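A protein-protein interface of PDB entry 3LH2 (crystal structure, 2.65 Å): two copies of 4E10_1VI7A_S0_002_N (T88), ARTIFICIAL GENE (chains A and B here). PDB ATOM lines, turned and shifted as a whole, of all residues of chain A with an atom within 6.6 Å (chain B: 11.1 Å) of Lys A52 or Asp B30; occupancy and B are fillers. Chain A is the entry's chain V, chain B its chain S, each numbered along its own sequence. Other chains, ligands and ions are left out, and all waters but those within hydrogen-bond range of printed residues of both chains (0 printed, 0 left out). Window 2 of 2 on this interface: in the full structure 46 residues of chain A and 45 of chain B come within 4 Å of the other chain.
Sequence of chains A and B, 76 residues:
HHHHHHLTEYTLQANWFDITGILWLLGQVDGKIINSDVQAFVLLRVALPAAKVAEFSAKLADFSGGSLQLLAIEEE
The backbone carbonyl oxygen (O) of Leu B26 is in hydrogen-bond range of the backbone NH (N) of Gly B31, at 2.7 Å.
The side-chain amino group (NZ) of Lys A52 lies within salt-bridge range of the side-chain carboxylate (OE2) of Glu A55, 3.9 Å away.
No position is printed for both chains.
Of the 15 pairs that touch across the chains among the printed residues, none has its exchanged pair printed and touching as well.
Of the 11 printed residues of chain A, 7 touch a printed residue of chain B.
Hydrophobic or aromatic side chains of chain B that line the printed part of chain A: Leu B7, Tyr B10, Leu B26, Val B29 and Ile B34.
The backbone carbonyl oxygen of Leu A48 sits at hydrogen-bond distance from the backbone NH of Thr B8, at 2.9 Å.
The backbone carbonyl oxygen of Ala A47 lies within hydrogen-bond range of the backbone NH of Lys B32, 2.8 Å away.
Among the printed residues, merely in contact across the chains: Ala A47 with Thr B8 (3.2 Å), Ala A47 with Gly B31 (3.3 Å), Ala A47 with Ile B34 (3.8 Å), Leu A48 with Leu B7 (3.7 Å), Pro A49 with Val B29 (3.6 Å), Pro A49 with Asp B30 (3.9 Å), Lys A52 with Val B29 (3.6 Å), Lys A52 with Asp B30 (3.8 Å), Val A53 with Tyr B10 (3.4 Å), Glu A55 with Val B29 (3.6 Å), Phe A56 with Leu B25 (3.95 Å), Phe A56 with Leu B26 (3.2 Å) and Phe A56 with Val B29 (3.7 Å).
Leu A48 touches two residues of chain B.
Lys A52 touches just these residues of chain B: Val B29 (3.6 Å) and Asp B30 (3.8 Å).
No residue of chain B comes within 4 Å of Ala A54.
Of the printed residues of chain B, Phe A56 touches Leu B25, Leu B26 and Val B29.
Printed residues of chain A within 4 Å of Thr B8: Ala A47 (3.2 Å) and Leu A48 (2.9 Å).
Gln B28 touches none of the printed residues of chain A.
Asp B30 touches just these residues of chain A: Pro A49 (3.9 Å) and Lys A52 (3.8 Å).
Printed residues of chain A within 4 Å of Gly B31: Ala A47.
Printed residues of chain A within 4 Å of Lys B32: Ala A47.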
ATOM      1  N   ALA A  47       4.993  -9.802  21.964  1.00  0.00           N
ATOM      2  CA  ALA A  47       5.995 -10.647  22.598  1.00  0.00           C
ATOM      3  C   ALA A  47       5.386 -11.340  23.811  1.00  0.00           C
ATOM      4  O   ALA A  47       4.801 -10.693  24.676  1.00  0.00           O
ATOM      5  CB  ALA A  47       7.210  -9.816  23.008  1.00  0.00           C
ATOM      6  N   LEU A  48       5.500 -12.663  23.857  1.00  0.00           N
ATOM      7  CA  LEU A  48       5.082 -13.415  25.043  1.00  0.00           C
ATOM      8  C   LEU A  48       5.965 -14.647  25.247  1.00  0.00           C
ATOM      9  O   LEU A  48       6.694 -15.040  24.345  1.00  0.00           O
ATOM     10  CB  LEU A  48       3.600 -13.789  24.960  1.00  0.00           C
ATOM     11  CG  LEU A  48       3.136 -14.698  23.828  1.00  0.00           C
ATOM     12  CD1 LEU A  48       1.868 -15.410  24.269  1.00  0.00           C
ATOM     13  CD2 LEU A  48       2.902 -13.923  22.543  1.00  0.00           C
ATOM     14  N   PRO A  49       5.918 -15.243  26.445  1.00  0.00           N
ATOM     15  CA  PRO A  49       6.750 -16.410  26.717  1.00  0.00           C
ATOM     16  C   PRO A  49       6.311 -17.615  25.908  1.00  0.00           C
ATOM     17  O   PRO A  49       5.118 -17.795  25.681  1.00  0.00           O
ATOM     18  CB  PRO A  49       6.522 -16.682  28.212  1.00  0.00           C
ATOM     19  CG  PRO A  49       5.786 -15.512  28.741  1.00  0.00           C
ATOM     20  CD  PRO A  49       5.085 -14.877  27.599  1.00  0.00           C
ATOM     21  N   ALA A  50       7.266 -18.443  25.500  1.00  0.00           N
ATOM     22  CA  ALA A  50       6.963 -19.633  24.700  1.00  0.00           C
ATOM     23  C   ALA A  50       5.872 -20.492  25.341  1.00  0.00           C
ATOM     24  O   ALA A  50       5.018 -21.033  24.648  1.00  0.00           O
ATOM     25  CB  ALA A  50       8.224 -20.454  24.477  1.00  0.00           C
ATOM     26  N   ALA A  51       5.893 -20.592  26.663  1.00  0.00           N
ATOM     27  CA  ALA A  51       4.919 -21.408  27.389  1.00  0.00           C
ATOM     28  C   ALA A  51       3.461 -20.937  27.256  1.00  0.00           C
ATOM     29  O   ALA A  51       2.546 -21.726  27.468  1.00  0.00           O
ATOM     30  CB  ALA A  51       5.309 -21.505  28.869  1.00  0.00           C
ATOM     31  N   LYS A  52       3.235 -19.670  26.913  1.00  0.00           N
ATOM     32  CA  LYS A  52       1.866 -19.139  26.873  1.00  0.00           C
ATOM     33  C   LYS A  52       1.275 -19.036  25.467  1.00  0.00           C
ATOM     34  O   LYS A  52       0.109 -18.698  25.316  1.00  0.00           O
ATOM     35  CB  LYS A  52       1.805 -17.754  27.524  1.00  0.00           C
ATOM     36  CG  LYS A  52       2.255 -17.699  28.974  1.00  0.00           C
ATOM     37  CD  LYS A  52       1.281 -18.400  29.901  1.00  0.00           C
ATOM     38  CE  LYS A  52       1.682 -18.220  31.360  1.00  0.00           C
ATOM     39  NZ  LYS A  52       0.653 -18.764  32.294  1.00  0.00           N
ATOM     40  N   VAL A  53       2.070 -19.333  24.444  1.00  0.00           N
ATOM     41  CA  VAL A  53       1.646 -19.132  23.058  1.00  0.00           C
ATOM     42  C   VAL A  53       0.378 -19.914  22.700  1.00  0.00           C
ATOM     43  O   VAL A  53      -0.472 -19.421  21.964  1.00  0.00           O
ATOM     44  CB  VAL A  53       2.775 -19.505  22.070  1.00  0.00           C
ATOM     45  CG1 VAL A  53       2.267 -19.490  20.638  1.00  0.00           C
ATOM     46  CG2 VAL A  53       3.954 -18.554  22.225  1.00  0.00           C
ATOM     47  N   ALA A  54       0.252 -21.129  23.219  1.00  0.00           N
ATOM     48  CA  ALA A  54      -0.904 -21.964  22.921  1.00  0.00           C
ATOM     49  C   ALA A  54      -2.156 -21.393  23.580  1.00  0.00           C
ATOM     50  O   ALA A  54      -3.200 -21.236  22.939  1.00  0.00           O
ATOM     51  CB  ALA A  54      -0.658 -23.393  23.391  1.00  0.00           C
ATOM     52  N   GLU A  55      -2.045 -21.082  24.865  1.00  0.00           N
ATOM     53  CA  GLU A  55      -3.157 -20.500  25.604  1.00  0.00           C
ATOM     54  C   GLU A  55      -3.631 -19.213  24.921  1.00  0.00           C
ATOM     55  O   GLU A  55      -4.830 -18.995  24.744  1.00  0.00           O
ATOM     56  CB  GLU A  55      -2.723 -20.214  27.040  1.00  0.00           C
ATOM     57  CG  GLU A  55      -3.823 -19.725  27.960  1.00  0.00           C
ATOM     58  CD  GLU A  55      -3.272 -19.180  29.265  1.00  0.00           C
ATOM     59  OE1 GLU A  55      -3.961 -18.367  29.911  1.00  0.00           O
ATOM     60  OE2 GLU A  55      -2.138 -19.553  29.638  1.00  0.00           O
ATOM     61  N   PHE A  56      -2.681 -18.370  24.535  1.00  0.00           N
ATOM     62  CA  PHE A  56      -2.982 -17.106  23.875  1.00  0.00           C
ATOM     63  C   PHE A  56      -3.653 -17.363  22.531  1.00  0.00           C
ATOM     64  O   PHE A  56      -4.713 -16.815  22.241  1.00  0.00           O
ATOM     65  CB  PHE A  56      -1.688 -16.311  23.679  1.00  0.00           C
ATOM     66  CG  PHE A  56      -1.895 -14.929  23.140  1.00  0.00           C
ATOM     67  CD1 PHE A  56      -1.371 -14.566  21.914  1.00  0.00           C
ATOM     68  CD2 PHE A  56      -2.601 -13.994  23.858  1.00  0.00           C
ATOM     69  CE1 PHE A  56      -1.555 -13.293  21.414  1.00  0.00           C
ATOM     70  CE2 PHE A  56      -2.786 -12.718  23.362  1.00  0.00           C
ATOM     71  CZ  PHE A  56      -2.263 -12.369  22.139  1.00  0.00           C
ATOM     72  N   SER A  57      -3.036 -18.219  21.727  1.00  0.00           N
ATOM     73  CA  SER A  57      -3.545 -18.546  20.399  1.00  0.00           C
ATOM     74  C   SER A  57      -4.965 -19.120  20.447  1.00  0.00           C
ATOM     75  O   SER A  57      -5.784 -18.838  19.562  1.00  0.00           O
ATOM     76  CB  SER A  57      -2.602 -19.539  19.714  1.00  0.00           C
ATOM     77  OG  SER A  57      -2.927 -19.716  18.349  1.00  0.00           O
ATOM     78  N   HIS B   6      13.990 -16.094  26.728  1.00  0.00           N
ATOM     79  CA  HIS B   6      13.403 -14.723  26.742  1.00  0.00           C
ATOM     80  C   HIS B   6      11.922 -14.791  26.379  1.00  0.00           C
ATOM     81  O   HIS B   6      11.209 -15.685  26.835  1.00  0.00           O
ATOM     82  CB  HIS B   6      14.154 -13.802  25.766  1.00  0.00           C
ATOM     83  N   LEU B   7      11.472 -13.837  25.566  1.00  0.00           N
ATOM     84  CA  LEU B   7      10.097 -13.800  25.080  1.00  0.00           C
ATOM     85  C   LEU B   7      10.137 -13.885  23.559  1.00  0.00           C
ATOM     86  O   LEU B   7      10.975 -13.244  22.928  1.00  0.00           O
ATOM     87  CB  LEU B   7       9.408 -12.502  25.524  1.00  0.00           C
ATOM     88  CG  LEU B   7       8.774 -12.470  26.927  1.00  0.00           C
ATOM     89  CD1 LEU B   7       9.797 -12.773  28.015  1.00  0.00           C
ATOM     90  CD2 LEU B   7       8.102 -11.127  27.198  1.00  0.00           C
ATOM     91  N   THR B   8       9.245 -14.676  22.968  1.00  0.00           N
ATOM     92  CA  THR B   8       9.208 -14.821  21.509  1.00  0.00           C
ATOM     93  C   THR B   8       8.234 -13.825  20.873  1.00  0.00           C
ATOM     94  O   THR B   8       7.241 -13.428  21.486  1.00  0.00           O
ATOM     95  CB  THR B   8       8.820 -16.254  21.070  1.00  0.00           C
ATOM     96  OG1 THR B   8       9.466 -17.216  21.913  1.00  0.00           O
ATOM     97  CG2 THR B   8       9.223 -16.496  19.612  1.00  0.00           C
ATOM     98  N   GLU B   9       8.527 -13.445  19.631  1.00  0.00           N
ATOM     99  CA  GLU B   9       7.780 -12.401  18.930  1.00  0.00           C
ATOM    100  C   GLU B   9       6.900 -12.956  17.810  1.00  0.00           C
ATOM    101  O   GLU B   9       7.325 -13.789  17.018  1.00  0.00           O
ATOM    102  CB  GLU B   9       8.746 -11.354  18.362  1.00  0.00           C
ATOM    103  CG  GLU B   9       9.668 -10.735  19.412  1.00  0.00           C
ATOM    104  CD  GLU B   9      10.390  -9.488  18.922  1.00  0.00           C
ATOM    105  OE1 GLU B   9      10.386  -9.217  17.706  1.00  0.00           O
ATOM    106  OE2 GLU B   9      10.963  -8.770  19.763  1.00  0.00           O
ATOM    107  N   TYR B  10       5.663 -12.479  17.756  1.00  0.00           N
ATOM    108  CA  TYR B  10       4.738 -12.849  16.695  1.00  0.00           C
ATOM    109  C   TYR B  10       4.100 -11.580  16.145  1.00  0.00           C
ATOM    110  O   TYR B  10       4.082 -10.547  16.815  1.00  0.00           O
ATOM    111  CB  TYR B  10       3.646 -13.777  17.230  1.00  0.00           C
ATOM    112  CG  TYR B  10       4.132 -15.115  17.746  1.00  0.00           C
ATOM    113  CD1 TYR B  10       4.735 -15.224  18.990  1.00  0.00           C
ATOM    114  CD2 TYR B  10       3.962 -16.278  16.999  1.00  0.00           C
ATOM    115  CE1 TYR B  10       5.172 -16.452  19.472  1.00  0.00           C
ATOM    116  CE2 TYR B  10       4.389 -17.510  17.472  1.00  0.00           C
ATOM    117  CZ  TYR B  10       4.992 -17.590  18.709  1.00  0.00           C
ATOM    118  OH  TYR B  10       5.424 -18.806  19.191  1.00  0.00           O
ATOM    119  N   ILE B  22      -7.457  -7.887  22.280  1.00  0.00           N
ATOM    120  CA  ILE B  22      -6.169  -8.525  22.088  1.00  0.00           C
ATOM    121  C   ILE B  22      -5.203  -8.037  23.167  1.00  0.00           C
ATOM    122  O   ILE B  22      -4.454  -8.825  23.732  1.00  0.00           O
ATOM    123  CB  ILE B  22      -5.643  -8.253  20.666  1.00  0.00           C
ATOM    124  CG1 ILE B  22      -6.524  -9.009  19.660  1.00  0.00           C
ATOM    125  CG2 ILE B  22      -4.178  -8.662  20.533  1.00  0.00           C
ATOM    126  CD1 ILE B  22      -6.271  -8.668  18.211  1.00  0.00           C
ATOM    127  N   LEU B  23      -5.254  -6.748  23.482  1.00  0.00           N
ATOM    128  CA  LEU B  23      -4.400  -6.192  24.521  1.00  0.00           C
ATOM    129  C   LEU B  23      -4.730  -6.763  25.893  1.00  0.00           C
ATOM    130  O   LEU B  23      -3.836  -7.044  26.684  1.00  0.00           O
ATOM    131  CB  LEU B  23      -4.499  -4.665  24.545  1.00  0.00           C
ATOM    132  CG  LEU B  23      -3.676  -3.971  23.453  1.00  0.00           C
ATOM    133  CD1 LEU B  23      -3.788  -2.456  23.550  1.00  0.00           C
ATOM    134  CD2 LEU B  23      -2.212  -4.402  23.535  1.00  0.00           C
ATOM    135  N   TRP B  24      -6.017  -6.938  26.166  1.00  0.00           N
ATOM    136  CA  TRP B  24      -6.472  -7.461  27.446  1.00  0.00           C
ATOM    137  C   TRP B  24      -6.020  -8.911  27.623  1.00  0.00           C
ATOM    138  O   TRP B  24      -5.527  -9.290  28.695  1.00  0.00           O
ATOM    139  CB  TRP B  24      -7.995  -7.354  27.539  1.00  0.00           C
ATOM    140  CG  TRP B  24      -8.563  -7.865  28.818  1.00  0.00           C
ATOM    141  CD1 TRP B  24      -8.673  -7.187  29.998  1.00  0.00           C
ATOM    142  CD2 TRP B  24      -9.112  -9.168  29.052  1.00  0.00           C
ATOM    143  NE1 TRP B  24      -9.248  -7.992  30.953  1.00  0.00           N
ATOM    144  CE2 TRP B  24      -9.524  -9.213  30.397  1.00  0.00           C
ATOM    145  CE3 TRP B  24      -9.291 -10.300  28.253  1.00  0.00           C
ATOM    146  CZ2 TRP B  24     -10.112 -10.345  30.960  1.00  0.00           C
ATOM    147  CZ3 TRP B  24      -9.872 -11.428  28.816  1.00  0.00           C
ATOM    148  CH2 TRP B  24     -10.279 -11.440  30.155  1.00  0.00           C
ATOM    149  N   LEU B  25      -6.189  -9.711  26.570  1.00  0.00           N
ATOM    150  CA  LEU B  25      -5.746 -11.109  26.573  1.00  0.00           C
ATOM    151  C   LEU B  25      -4.230 -11.196  26.710  1.00  0.00           C
ATOM    152  O   LEU B  25      -3.713 -12.056  27.427  1.00  0.00           O
ATOM    153  CB  LEU B  25      -6.180 -11.832  25.289  1.00  0.00           C
ATOM    154  CG  LEU B  25      -7.670 -12.186  25.173  1.00  0.00           C
ATOM    155  CD1 LEU B  25      -8.005 -12.783  23.802  1.00  0.00           C
ATOM    156  CD2 LEU B  25      -8.086 -13.134  26.295  1.00  0.00           C
ATOM    157  N   LEU B  26      -3.528 -10.295  26.025  1.00  0.00           N
ATOM    158  CA  LEU B  26      -2.072 -10.269  26.056  1.00  0.00           C
ATOM    159  C   LEU B  26      -1.569 -10.056  27.483  1.00  0.00           C
ATOM    160  O   LEU B  26      -0.571 -10.644  27.891  1.00  0.00           O
ATOM    161  CB  LEU B  26      -1.544  -9.169  25.128  1.00  0.00           C
ATOM    162  CG  LEU B  26      -0.163  -9.341  24.487  1.00  0.00           C
ATOM    163  CD1 LEU B  26      -0.054 -10.689  23.801  1.00  0.00           C
ATOM    164  CD2 LEU B  26       0.114  -8.211  23.492  1.00  0.00           C
ATOM    165  N   GLY B  27      -2.275  -9.225  28.242  1.00  0.00           N
ATOM    166  CA  GLY B  27      -1.910  -8.953  29.630  1.00  0.00           C
ATOM    167  C   GLY B  27      -2.080 -10.166  30.527  1.00  0.00           C
ATOM    168  O   GLY B  27      -1.290 -10.376  31.447  1.00  0.00           O
ATOM    169  N   GLN B  28      -3.111 -10.967  30.248  1.00  0.00           N
ATOM    170  CA  GLN B  28      -3.422 -12.160  31.035  1.00  0.00           C
ATOM    171  C   GLN B  28      -2.415 -13.289  30.839  1.00  0.00           C
ATOM    172  O   GLN B  28      -2.446 -14.268  31.576  1.00  0.00           O
ATOM    173  CB  GLN B  28      -4.823 -12.681  30.691  1.00  0.00           C
ATOM    174  CG  GLN B  28      -5.961 -11.766  31.143  1.00  0.00           C
ATOM    175  CD  GLN B  28      -6.151 -11.755  32.657  1.00  0.00           C
ATOM    176  OE1 GLN B  28      -6.196 -12.809  33.299  1.00  0.00           O
ATOM    177  NE2 GLN B  28      -6.272 -10.564  33.229  1.00  0.00           N
ATOM    178  N   VAL B  29      -1.538 -13.160  29.846  1.00  0.00           N
ATOM    179  CA  VAL B  29      -0.517 -14.174  29.582  1.00  0.00           C
ATOM    180  C   VAL B  29       0.900 -13.575  29.612  1.00  0.00           C
ATOM    181  O   VAL B  29       1.821 -14.077  28.962  1.00  0.00           O
ATOM    182  CB  VAL B  29      -0.782 -14.881  28.239  1.00  0.00           C
ATOM    183  CG1 VAL B  29      -2.023 -15.749  28.342  1.00  0.00           C
ATOM    184  CG2 VAL B  29      -0.932 -13.867  27.116  1.00  0.00           C
ATOM    185  N   ASP B  30       1.059 -12.499  30.378  1.00  0.00           N
ATOM    186  CA  ASP B  30       2.355 -11.850  30.580  1.00  0.00           C
ATOM    187  C   ASP B  30       2.964 -11.341  29.273  1.00  0.00           C
ATOM    188  O   ASP B  30       4.183 -11.346  29.106  1.00  0.00           O
ATOM    189  CB  ASP B  30       3.326 -12.807  31.281  1.00  0.00           C
ATOM    190  CG  ASP B  30       2.714 -13.465  32.514  1.00  0.00           C
ATOM    191  OD1 ASP B  30       2.363 -12.737  33.467  1.00  0.00           O
ATOM    192  OD2 ASP B  30       2.584 -14.713  32.534  1.00  0.00           O
ATOM    193  N   GLY B  31       2.115 -10.884  28.358  1.00  0.00           N
ATOM    194  CA  GLY B  31       2.573 -10.422  27.049  1.00  0.00           C
ATOM    195  C   GLY B  31       2.781  -8.921  26.959  1.00  0.00           C
ATOM    196  O   GLY B  31       2.280  -8.163  27.788  1.00  0.00           O
ATOM    197  N   LYS B  32       3.527  -8.501  25.943  1.00  0.00           N
ATOM    198  CA  LYS B  32       3.798  -7.090  25.697  1.00  0.00           C
ATOM    199  C   LYS B  32       3.618  -6.754  24.207  1.00  0.00           C
ATOM    200  O   LYS B  32       3.804  -7.613  23.338  1.00  0.00           O
ATOM    201  CB  LYS B  32       5.228  -6.742  26.127  1.00  0.00           C
ATOM    202  CG  LYS B  32       5.480  -6.807  27.631  1.00  0.00           C
ATOM    203  CD  LYS B  32       6.000  -8.170  28.082  1.00  0.00           C
ATOM    204  N   ILE B  33       3.255  -5.504  23.919  1.00  0.00           N
ATOM    205  CA  ILE B  33       3.212  -5.016  22.543  1.00  0.00           C
ATOM    206  C   ILE B  33       4.553  -4.387  22.219  1.00  0.00           C
ATOM    207  O   ILE B  33       4.965  -3.452  22.888  1.00  0.00           O
ATOM    208  CB  ILE B  33       2.106  -3.952  22.330  1.00  0.00           C
ATOM    209  CG1 ILE B  33       0.718  -4.568  22.510  1.00  0.00           C
ATOM    210  CG2 ILE B  33       2.214  -3.355  20.941  1.00  0.00           C
ATOM    211  N   ILE B  34       5.243  -4.899  21.207  1.00  0.00           N
ATOM    212  CA  ILE B  34       6.546  -4.353  20.835  1.00  0.00           C
ATOM    213  C   ILE B  34       6.400  -3.234  19.810  1.00  0.00           C
ATOM    214  O   ILE B  34       7.159  -2.266  19.831  1.00  0.00           O
ATOM    215  CB  ILE B  34       7.487  -5.438  20.260  1.00  0.00           C
ATOM    216  CG1 ILE B  34       7.906  -6.425  21.351  1.00  0.00           C
ATOM    217  CG2 ILE B  34       8.733  -4.798  19.661  1.00  0.00           C
ATOM    218  CD1 ILE B  34       8.889  -5.837  22.379  1.00  0.00           C
